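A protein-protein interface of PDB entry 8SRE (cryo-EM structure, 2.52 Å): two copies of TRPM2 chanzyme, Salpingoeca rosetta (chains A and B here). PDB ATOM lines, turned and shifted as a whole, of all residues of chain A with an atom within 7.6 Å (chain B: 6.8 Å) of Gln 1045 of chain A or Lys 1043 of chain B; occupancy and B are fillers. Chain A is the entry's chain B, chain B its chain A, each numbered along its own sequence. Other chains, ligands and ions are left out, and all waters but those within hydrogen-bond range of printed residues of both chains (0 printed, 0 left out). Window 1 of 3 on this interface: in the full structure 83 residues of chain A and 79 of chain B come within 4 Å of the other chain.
Of the 19 printed residues of chain A, 3 touch a printed residue of chain B.
Hydrophobic or aromatic side chains of chain A within 4 Å of the printed part of chain B: Tyr 1041.
Printed residues of chain B that touch a printed residue of chain A: Asn 1038, Asp 1039 and Lys 1043.
Among the printed residues, 4 pairs touch across the chains.
OD1 of Asn 1038 of chain B lies close to ND2 of Asn 1038 of chain A (3.4 Å).
NE2 of Gln 1045 of chain A is in hydrogen-bond range of OD2 of Asp 1039 of chain B (2.9 Å).
Met 930 of chain A touches none of the printed residues of chain B.
Printed residues of chain B within 4 Å of Gln 1045 of chain A: Asp 1039 and Lys 1043.
Asp 1050 of chain A touches none of the printed residues of chain B.
Of the printed residues of chain A, Asn 1038 of chain B touches Asn 1038.
Of the printed residues of chain A, Asp 1039 of chain B touches Tyr 1041 and Gln 1045.
Lys 1043 of chain B touches one residue of chain A.
The nearest residue of chain B that does not touch Gln 1045 of chain A is Thr 1040 of chain B (6.7 Å).
The nearest residue of chain A that does not touch Lys 1043 of chain B is Glu 1046 of chain A (6.4 Å).
The nearest printed residue of chain A that does not touch Asp 1039 of chain B is Met 1042 of chain A (5.0 Å).
Asn 1038 of chain A touches its own counterpart, Asn 1038 of chain B.
Tyr 1041 of chain A touches Asp 1039 of chain B, but with the chains exchanged Asp 1039 of chain A does not touch Tyr 1041 of chain B (13.4 Å).
Gln 1045 of chain A touches Asp 1039 of chain B, but with the chains exchanged Asp 1039 of chain A does not touch Gln 1045 of chain B (16.6 Å).
Gln 1045 of chain A touches Lys 1043 of chain B, but with the chains exchanged Lys 1043 of chain A does not touch Gln 1045 of chain B (17.8 Å).
10 positions are printed for both chains.
Of the 4 pairs that touch across the chains among the printed residues, 1 has its exchanged pair printed and touching as well.
Among the printed residues, merely in contact across the chains: Tyr 1041 of chain A with Asp 1039 of chain B (3.5 Å) and Gln 1045 of chain A with Lys 1043 of chain B (3.97 Å).
The side-chain carboxylate (OD1) of Asp 1039 of chain B lies within salt-bridge range of the side-chain amino group (NZ) of Lys 1043 of chain B, 3.5 Å away.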
ATOM      1  N   PRO A 926      13.368   6.145  -9.904  1.00  0.00           N
ATOM      2  CA  PRO A 926      14.191   4.987  -9.463  1.00  0.00           C
ATOM      3  C   PRO A 926      14.181   4.723  -7.957  1.00  0.00           C
ATOM      4  O   PRO A 926      14.343   3.565  -7.559  1.00  0.00           O
ATOM      5  CB  PRO A 926      15.592   5.306 -10.001  1.00  0.00           C
ATOM      6  CG  PRO A 926      15.359   6.191 -11.104  1.00  0.00           C
ATOM      7  CD  PRO A 926      14.207   7.016 -10.767  1.00  0.00           C
ATOM      8  N   LYS A 927      14.047   5.777  -7.135  1.00  0.00           N
ATOM      9  CA  LYS A 927      13.938   5.640  -5.685  1.00  0.00           C
ATOM     10  C   LYS A 927      12.628   4.959  -5.294  1.00  0.00           C
ATOM     11  O   LYS A 927      12.582   4.254  -4.281  1.00  0.00           O
ATOM     12  CB  LYS A 927      13.996   7.004  -5.020  1.00  0.00           C
ATOM     13  CG  LYS A 927      15.350   7.622  -4.998  1.00  0.00           C
ATOM     14  CD  LYS A 927      16.490   6.816  -4.530  1.00  0.00           C
ATOM     15  CE  LYS A 927      17.697   7.367  -5.259  1.00  0.00           C
ATOM     16  NZ  LYS A 927      17.808   8.855  -5.229  1.00  0.00           N
ATOM     17  N   ILE A 929      11.026   2.742  -7.271  1.00  0.00           N
ATOM     18  CA  ILE A 929      11.288   1.350  -7.681  1.00  0.00           C
ATOM     19  C   ILE A 929      12.160   0.646  -6.641  1.00  0.00           C
ATOM     20  O   ILE A 929      11.913  -0.528  -6.277  1.00  0.00           O
ATOM     21  CB  ILE A 929      11.845   1.314  -9.117  1.00  0.00           C
ATOM     22  CG1 ILE A 929      10.749   1.783 -10.060  1.00  0.00           C
ATOM     23  CG2 ILE A 929      12.421  -0.002  -9.545  1.00  0.00           C
ATOM     24  CD1 ILE A 929      11.235   2.409 -11.220  1.00  0.00           C
ATOM     25  N   MET A 930      13.160   1.393  -6.137  1.00  0.00           N
ATOM     26  CA  MET A 930      14.049   0.974  -5.064  1.00  0.00           C
ATOM     27  C   MET A 930      13.294   0.709  -3.764  1.00  0.00           C
ATOM     28  O   MET A 930      13.555  -0.316  -3.150  1.00  0.00           O
ATOM     29  CB  MET A 930      15.097   2.046  -4.800  1.00  0.00           C
ATOM     30  CG  MET A 930      16.279   1.532  -4.025  1.00  0.00           C
ATOM     31  SD  MET A 930      17.503   0.704  -5.047  1.00  0.00           S
ATOM     32  CE  MET A 930      17.679   1.920  -6.348  1.00  0.00           C
ATOM     33  N   ASN A1038      21.740  -1.552   2.390  1.00  0.00           N
ATOM     34  CA  ASN A1038      22.942  -1.091   1.680  1.00  0.00           C
ATOM     35  C   ASN A1038      23.371  -2.043   0.571  1.00  0.00           C
ATOM     36  O   ASN A1038      23.661  -1.602  -0.559  1.00  0.00           O
ATOM     37  CB  ASN A1038      24.092  -0.942   2.658  1.00  0.00           C
ATOM     38  CG  ASN A1038      24.138   0.396   3.295  1.00  0.00           C
ATOM     39  OD1 ASN A1038      23.904   0.556   4.489  1.00  0.00           O
ATOM     40  ND2 ASN A1038      24.451   1.378   2.504  1.00  0.00           N
ATOM     41  N   ASP A1039      23.335  -3.351   0.885  1.00  0.00           N
ATOM     42  CA  ASP A1039      23.658  -4.425  -0.053  1.00  0.00           C
ATOM     43  C   ASP A1039      22.659  -4.504  -1.194  1.00  0.00           C
ATOM     44  O   ASP A1039      23.060  -4.648  -2.361  1.00  0.00           O
ATOM     45  CB  ASP A1039      23.713  -5.745   0.675  1.00  0.00           C
ATOM     46  CG  ASP A1039      24.061  -6.894  -0.238  1.00  0.00           C
ATOM     47  OD1 ASP A1039      25.135  -6.844  -0.866  1.00  0.00           O
ATOM     48  OD2 ASP A1039      23.256  -7.841  -0.338  1.00  0.00           O
ATOM     49  N   THR A1040      21.357  -4.421  -0.843  1.00  0.00           N
ATOM     50  CA  THR A1040      20.231  -4.474  -1.772  1.00  0.00           C
ATOM     51  C   THR A1040      20.259  -3.305  -2.743  1.00  0.00           C
ATOM     52  O   THR A1040      20.111  -3.541  -3.948  1.00  0.00           O
ATOM     53  CB  THR A1040      18.932  -4.494  -0.967  1.00  0.00           C
ATOM     54  OG1 THR A1040      18.899  -5.679  -0.166  1.00  0.00           O
ATOM     55  CG2 THR A1040      17.678  -4.501  -1.836  1.00  0.00           C
ATOM     56  N   TYR A1041      20.574  -2.086  -2.223  1.00  0.00           N
ATOM     57  CA  TYR A1041      20.705  -0.823  -2.972  1.00  0.00           C
ATOM     58  C   TYR A1041      21.793  -0.927  -4.043  1.00  0.00           C
ATOM     59  O   TYR A1041      21.548  -0.569  -5.214  1.00  0.00           O
ATOM     60  CB  TYR A1041      20.978   0.336  -2.001  1.00  0.00           C
ATOM     61  CG  TYR A1041      20.779   1.726  -2.588  1.00  0.00           C
ATOM     62  CD1 TYR A1041      21.829   2.425  -3.233  1.00  0.00           C
ATOM     63  CD2 TYR A1041      19.519   2.345  -2.491  1.00  0.00           C
ATOM     64  CE1 TYR A1041      21.615   3.667  -3.783  1.00  0.00           C
ATOM     65  CE2 TYR A1041      19.302   3.613  -3.044  1.00  0.00           C
ATOM     66  CZ  TYR A1041      20.380   4.253  -3.664  1.00  0.00           C
ATOM     67  OH  TYR A1041      20.263   5.481  -4.229  1.00  0.00           O
ATOM     68  N   MET A1042      23.009  -1.377  -3.623  1.00  0.00           N
ATOM     69  CA  MET A1042      24.147  -1.601  -4.532  1.00  0.00           C
ATOM     70  C   MET A1042      23.844  -2.673  -5.589  1.00  0.00           C
ATOM     71  O   MET A1042      24.362  -2.605  -6.709  1.00  0.00           O
ATOM     72  CB  MET A1042      25.418  -1.968  -3.764  1.00  0.00           C
ATOM     73  CG  MET A1042      25.985  -0.860  -2.897  1.00  0.00           C
ATOM     74  SD  MET A1042      27.526  -1.331  -2.078  1.00  0.00           S
ATOM     75  CE  MET A1042      26.941  -2.445  -0.810  1.00  0.00           C
ATOM     76  N   LYS A1043      23.027  -3.679  -5.235  1.00  0.00           N
ATOM     77  CA  LYS A1043      22.700  -4.754  -6.167  1.00  0.00           C
ATOM     78  C   LYS A1043      21.705  -4.294  -7.238  1.00  0.00           C
ATOM     79  O   LYS A1043      21.860  -4.653  -8.411  1.00  0.00           O
ATOM     80  CB  LYS A1043      22.161  -5.980  -5.433  1.00  0.00           C
ATOM     81  CG  LYS A1043      23.239  -6.878  -4.856  1.00  0.00           C
ATOM     82  CD  LYS A1043      22.634  -8.009  -4.041  1.00  0.00           C
ATOM     83  CE  LYS A1043      23.651  -9.089  -3.679  1.00  0.00           C
ATOM     84  NZ  LYS A1043      25.074  -8.661  -3.826  1.00  0.00           N
ATOM     85  N   VAL A1044      20.683  -3.503  -6.880  1.00  0.00           N
ATOM     86  CA  VAL A1044      19.545  -3.332  -7.796  1.00  0.00           C
ATOM     87  C   VAL A1044      19.378  -1.891  -8.296  1.00  0.00           C
ATOM     88  O   VAL A1044      18.347  -1.600  -8.936  1.00  0.00           O
ATOM     89  CB  VAL A1044      18.205  -3.867  -7.210  1.00  0.00           C
ATOM     90  CG1 VAL A1044      18.275  -5.357  -6.862  1.00  0.00           C
ATOM     91  CG2 VAL A1044      17.564  -3.031  -6.036  1.00  0.00           C
ATOM     92  N   GLN A1045      20.390  -1.006  -8.091  1.00  0.00           N
ATOM     93  CA  GLN A1045      20.360   0.385  -8.591  1.00  0.00           C
ATOM     94  C   GLN A1045      20.307   0.515 -10.128  1.00  0.00           C
ATOM     95  O   GLN A1045      19.499   1.300 -10.658  1.00  0.00           O
ATOM     96  CB  GLN A1045      21.590   1.114  -8.058  1.00  0.00           C
ATOM     97  CG  GLN A1045      21.403   2.577  -7.786  1.00  0.00           C
ATOM     98  CD  GLN A1045      22.668   3.208  -7.256  1.00  0.00           C
ATOM     99  OE1 GLN A1045      23.564   2.512  -6.777  1.00  0.00           O
ATOM    100  NE2 GLN A1045      22.750   4.529  -7.333  1.00  0.00           N
ATOM    101  N   GLU A1046      21.115  -0.286 -10.846  1.00  0.00           N
ATOM    102  CA  GLU A1046      21.149  -0.268 -12.315  1.00  0.00           C
ATOM    103  C   GLU A1046      19.874  -0.863 -12.922  1.00  0.00           C
ATOM    104  O   GLU A1046      19.365  -0.367 -13.942  1.00  0.00           O
ATOM    105  CB  GLU A1046      22.379  -1.022 -12.813  1.00  0.00           C
ATOM    106  CG  GLU A1046      23.689  -0.356 -12.448  1.00  0.00           C
ATOM    107  CD  GLU A1046      24.078   0.731 -13.425  1.00  0.00           C
ATOM    108  OE1 GLU A1046      23.742   0.607 -14.621  1.00  0.00           O
ATOM    109  OE2 GLU A1046      24.721   1.713 -12.997  1.00  0.00           O
ATOM    110  N   ALA A1047      19.374  -1.938 -12.289  1.00  0.00           N
ATOM    111  CA  ALA A1047      18.108  -2.578 -12.639  1.00  0.00           C
ATOM    112  C   ALA A1047      16.915  -1.656 -12.414  1.00  0.00           C
ATOM    113  O   ALA A1047      15.934  -1.724 -13.167  1.00  0.00           O
ATOM    114  CB  ALA A1047      17.939  -3.868 -11.840  1.00  0.00           C
ATOM    115  N   ALA A1048      16.965  -0.849 -11.339  1.00  0.00           N
ATOM    116  CA  ALA A1048      15.947   0.165 -11.058  1.00  0.00           C
ATOM    117  C   ALA A1048      15.913   1.254 -12.122  1.00  0.00           C
ATOM    118  O   ALA A1048      14.825   1.742 -12.460  1.00  0.00           O
ATOM    119  CB  ALA A1048      16.184   0.777  -9.681  1.00  0.00           C
ATOM    120  N   GLU A1049      17.101   1.686 -12.600  1.00  0.00           N
ATOM    121  CA  GLU A1049      17.199   2.655 -13.706  1.00  0.00           C
ATOM    122  C   GLU A1049      16.618   2.101 -15.013  1.00  0.00           C
ATOM    123  O   GLU A1049      15.914   2.820 -15.741  1.00  0.00           O
ATOM    124  CB  GLU A1049      18.642   3.109 -13.915  1.00  0.00           C
ATOM    125  CG  GLU A1049      19.206   3.911 -12.769  1.00  0.00           C
ATOM    126  CD  GLU A1049      18.907   5.385 -12.891  1.00  0.00           C
ATOM    127  OE1 GLU A1049      18.610   5.841 -14.014  1.00  0.00           O
ATOM    128  OE2 GLU A1049      18.961   6.091 -11.863  1.00  0.00           O
ATOM    129  N   ASP A1050      16.937   0.824 -15.322  1.00  0.00           N
ATOM    130  CA  ASP A1050      16.417   0.119 -16.506  1.00  0.00           C
ATOM    131  C   ASP A1050      14.897  -0.071 -16.451  1.00  0.00           C
ATOM    132  O   ASP A1050      14.203   0.098 -17.470  1.00  0.00           O
ATOM    133  CB  ASP A1050      17.114  -1.230 -16.643  1.00  0.00           C
ATOM    134  CG  ASP A1050      18.544  -1.100 -17.132  1.00  0.00           C
ATOM    135  OD1 ASP A1050      18.896  -0.035 -17.676  1.00  0.00           O
ATOM    136  OD2 ASP A1050      19.319  -2.065 -16.967  1.00  0.00           O
ATOM    137  N   LEU A1051      14.384  -0.463 -15.270  1.00  0.00           N
ATOM    138  CA  LEU A1051      12.954  -0.641 -15.017  1.00  0.00           C
ATOM    139  C   LEU A1051      12.209   0.694 -15.096  1.00  0.00           C
ATOM    140  O   LEU A1051      11.055   0.716 -15.542  1.00  0.00           O
ATOM    141  CB  LEU A1051      12.752  -1.401 -13.703  1.00  0.00           C
ATOM    142  CG  LEU A1051      11.359  -1.710 -13.158  1.00  0.00           C
ATOM    143  CD1 LEU A1051      10.559  -2.414 -14.191  1.00  0.00           C
ATOM    144  CD2 LEU A1051      11.514  -2.702 -12.042  1.00  0.00           C
ATOM    145  N   ARG A1053      13.209   3.178 -17.040  1.00  0.00           N
ATOM    146  CA  ARG A1053      13.180   3.428 -18.480  1.00  0.00           C
ATOM    147  C   ARG A1053      12.077   2.626 -19.186  1.00  0.00           C
ATOM    148  O   ARG A1053      11.570   3.078 -20.218  1.00  0.00           O
ATOM    149  CB  ARG A1053      14.559   3.176 -19.080  1.00  0.00           C
ATOM    150  CG  ARG A1053      15.512   4.314 -18.756  1.00  0.00           C
ATOM    151  CD  ARG A1053      16.836   4.196 -19.459  1.00  0.00           C
ATOM    152  NE  ARG A1053      17.683   3.198 -18.824  1.00  0.00           N
ATOM    153  CZ  ARG A1053      18.727   3.482 -18.060  1.00  0.00           C
ATOM    154  NH1 ARG A1053      19.075   4.733 -17.808  1.00  0.00           N
ATOM    155  NH2 ARG A1053      19.435   2.489 -17.531  1.00  0.00           N
ATOM    156  N   ASN B1038      25.396   6.436   1.766  1.00  0.00           N
ATOM    157  CA  ASN B1038      26.595   5.600   1.616  1.00  0.00           C
ATOM    158  C   ASN B1038      27.046   5.472   0.167  1.00  0.00           C
ATOM    159  O   ASN B1038      28.246   5.628  -0.135  1.00  0.00           O
ATOM    160  CB  ASN B1038      26.324   4.210   2.160  1.00  0.00           C
ATOM    161  CG  ASN B1038      26.607   4.092   3.611  1.00  0.00           C
ATOM    162  OD1 ASN B1038      25.714   3.925   4.436  1.00  0.00           O
ATOM    163  ND2 ASN B1038      27.861   4.169   3.941  1.00  0.00           N
ATOM    164  N   ASP B1039      26.064   5.263  -0.729  1.00  0.00           N
ATOM    165  CA  ASP B1039      26.281   5.163  -2.172  1.00  0.00           C
ATOM    166  C   ASP B1039      26.765   6.475  -2.766  1.00  0.00           C
ATOM    167  O   ASP B1039      27.703   6.479  -3.578  1.00  0.00           O
ATOM    168  CB  ASP B1039      25.009   4.729  -2.855  1.00  0.00           C
ATOM    169  CG  ASP B1039      25.173   4.591  -4.347  1.00  0.00           C
ATOM    170  OD1 ASP B1039      26.037   3.803  -4.775  1.00  0.00           O
ATOM    171  OD2 ASP B1039      24.448   5.279  -5.094  1.00  0.00           O
ATOM    172  N   THR B1040      26.109   7.584  -2.358  1.00  0.00           N
ATOM    173  CA  THR B1040      26.405   8.945  -2.796  1.00  0.00           C
ATOM    174  C   THR B1040      27.804   9.369  -2.382  1.00  0.00           C
ATOM    175  O   THR B1040      28.535   9.890  -3.234  1.00  0.00           O
ATOM    176  CB  THR B1040      25.348   9.887  -2.221  1.00  0.00           C
ATOM    177  OG1 THR B1040      24.067   9.524  -2.744  1.00  0.00           O
ATOM    178  CG2 THR B1040      25.581  11.353  -2.576  1.00  0.00           C
ATOM    179  N   TYR B1041      28.199   9.026  -1.124  1.00  0.00           N
ATOM    180  CA  TYR B1041      29.518   9.289  -0.520  1.00  0.00           C
ATOM    181  C   TYR B1041      30.635   8.621  -1.324  1.00  0.00           C
ATOM    182  O   TYR B1041      31.641   9.283  -1.658  1.00  0.00           O
ATOM    183  CB  TYR B1041      29.523   8.827   0.945  1.00  0.00           C
ATOM    184  CG  TYR B1041      30.680   9.357   1.781  1.00  0.00           C
ATOM    185  CD1 TYR B1041      31.912   8.665   1.880  1.00  0.00           C
ATOM    186  CD2 TYR B1041      30.530  10.568   2.482  1.00  0.00           C
ATOM    187  CE1 TYR B1041      32.952   9.182   2.616  1.00  0.00           C
ATOM    188  CE2 TYR B1041      31.586  11.091   3.238  1.00  0.00           C
ATOM    189  CZ  TYR B1041      32.776  10.359   3.299  1.00  0.00           C
ATOM    190  OH  TYR B1041      33.853  10.788   4.005  1.00  0.00           O
ATOM    191  N   MET B1042      30.473   7.294  -1.592  1.00  0.00           N
ATOM    192  CA  MET B1042      31.419   6.512  -2.408  1.00  0.00           C
ATOM    193  C   MET B1042      31.517   7.041  -3.847  1.00  0.00           C
ATOM    194  O   MET B1042      32.578   6.940  -4.474  1.00  0.00           O
ATOM    195  CB  MET B1042      31.058   5.026  -2.420  1.00  0.00           C
ATOM    196  CG  MET B1042      31.213   4.319  -1.086  1.00  0.00           C
ATOM    197  SD  MET B1042      30.845   2.553  -1.184  1.00  0.00           S
ATOM    198  CE  MET B1042      29.065   2.555  -1.327  1.00  0.00           C
ATOM    199  N   LYS B1043      30.411   7.580  -4.387  1.00  0.00           N
ATOM    200  CA  LYS B1043      30.406   8.087  -5.755  1.00  0.00           C
ATOM    201  C   LYS B1043      31.140   9.428  -5.867  1.00  0.00           C
ATOM    202  O   LYS B1043      31.878   9.641  -6.835  1.00  0.00           O
ATOM    203  CB  LYS B1043      28.982   8.215  -6.293  1.00  0.00           C
ATOM    204  CG  LYS B1043      28.404   6.918  -6.828  1.00  0.00           C
ATOM    205  CD  LYS B1043      26.950   7.091  -7.235  1.00  0.00           C
ATOM    206  CE  LYS B1043      26.412   5.904  -8.030  1.00  0.00           C
ATOM    207  NZ  LYS B1043      27.241   4.667  -7.917  1.00  0.00           N
ATOM    208  N   VAL B1044      30.969  10.347  -4.906  1.00  0.00           N
ATOM    209  CA  VAL B1044      31.376  11.738  -5.152  1.00  0.00           C
ATOM    210  C   VAL B1044      32.506  12.214  -4.230  1.00  0.00           C
ATOM    211  O   VAL B1044      32.808  13.424  -4.236  1.00  0.00           O
ATOM    212  CB  VAL B1044      30.182  12.738  -5.118  1.00  0.00           C
ATOM    213  CG1 VAL B1044      29.108  12.398  -6.156  1.00  0.00           C
ATOM    214  CG2 VAL B1044      29.547  13.029  -3.705  1.00  0.00           C
ATOM    215  N   GLN B1045      33.186  11.291  -3.499  1.00  0.00           N
ATOM    216  CA  GLN B1045      34.334  11.633  -2.632  1.00  0.00           C
ATOM    217  C   GLN B1045      35.554  12.214  -3.379  1.00  0.00           C
ATOM    218  O   GLN B1045      36.124  13.231  -2.942  1.00  0.00           O
ATOM    219  CB  GLN B1045      34.751  10.378  -1.870  1.00  0.00           C
ATOM    220  CG  GLN B1045      35.303  10.614  -0.495  1.00  0.00           C
ATOM    221  CD  GLN B1045      35.679   9.319   0.181  1.00  0.00           C
ATOM    222  OE1 GLN B1045      35.227   8.247  -0.221  1.00  0.00           O
ATOM    223  NE2 GLN B1045      36.505   9.407   1.214  1.00  0.00           N
ATOM    224  N   GLU B1046      35.920  11.616  -4.527  1.00  0.00           N
ATOM    225  CA  GLU B1046      37.053  12.082  -5.338  1.00  0.00           C
ATOM    226  C   GLU B1046      36.752  13.416  -6.027  1.00  0.00           C
ATOM    227  O   GLU B1046      37.631  14.289  -6.134  1.00  0.00           O
ATOM    228  CB  GLU B1046      37.421  11.020  -6.370  1.00  0.00           C
ATOM    229  CG  GLU B1046      37.958   9.741  -5.762  1.00  0.00           C
ATOM    230  CD  GLU B1046      39.437   9.820  -5.459  1.00  0.00           C
ATOM    231  OE1 GLU B1046      40.161  10.525  -6.193  1.00  0.00           O
ATOM    232  OE2 GLU B1046      39.879   9.177  -4.482  1.00  0.00           O
ATOM    233  N   ALA B1047      35.503  13.558  -6.501  1.00  0.00           N
ATOM    234  CA  ALA B1047      34.984  14.794  -7.085  1.00  0.00           C
ATOM    235  C   ALA B1047      34.930  15.931  -6.071  1.00  0.00           C
ATOM    236  O   ALA B1047      35.132  17.095  -6.440  1.00  0.00           O
ATOM    237  CB  ALA B1047      33.599  14.547  -7.679  1.00  0.00           C
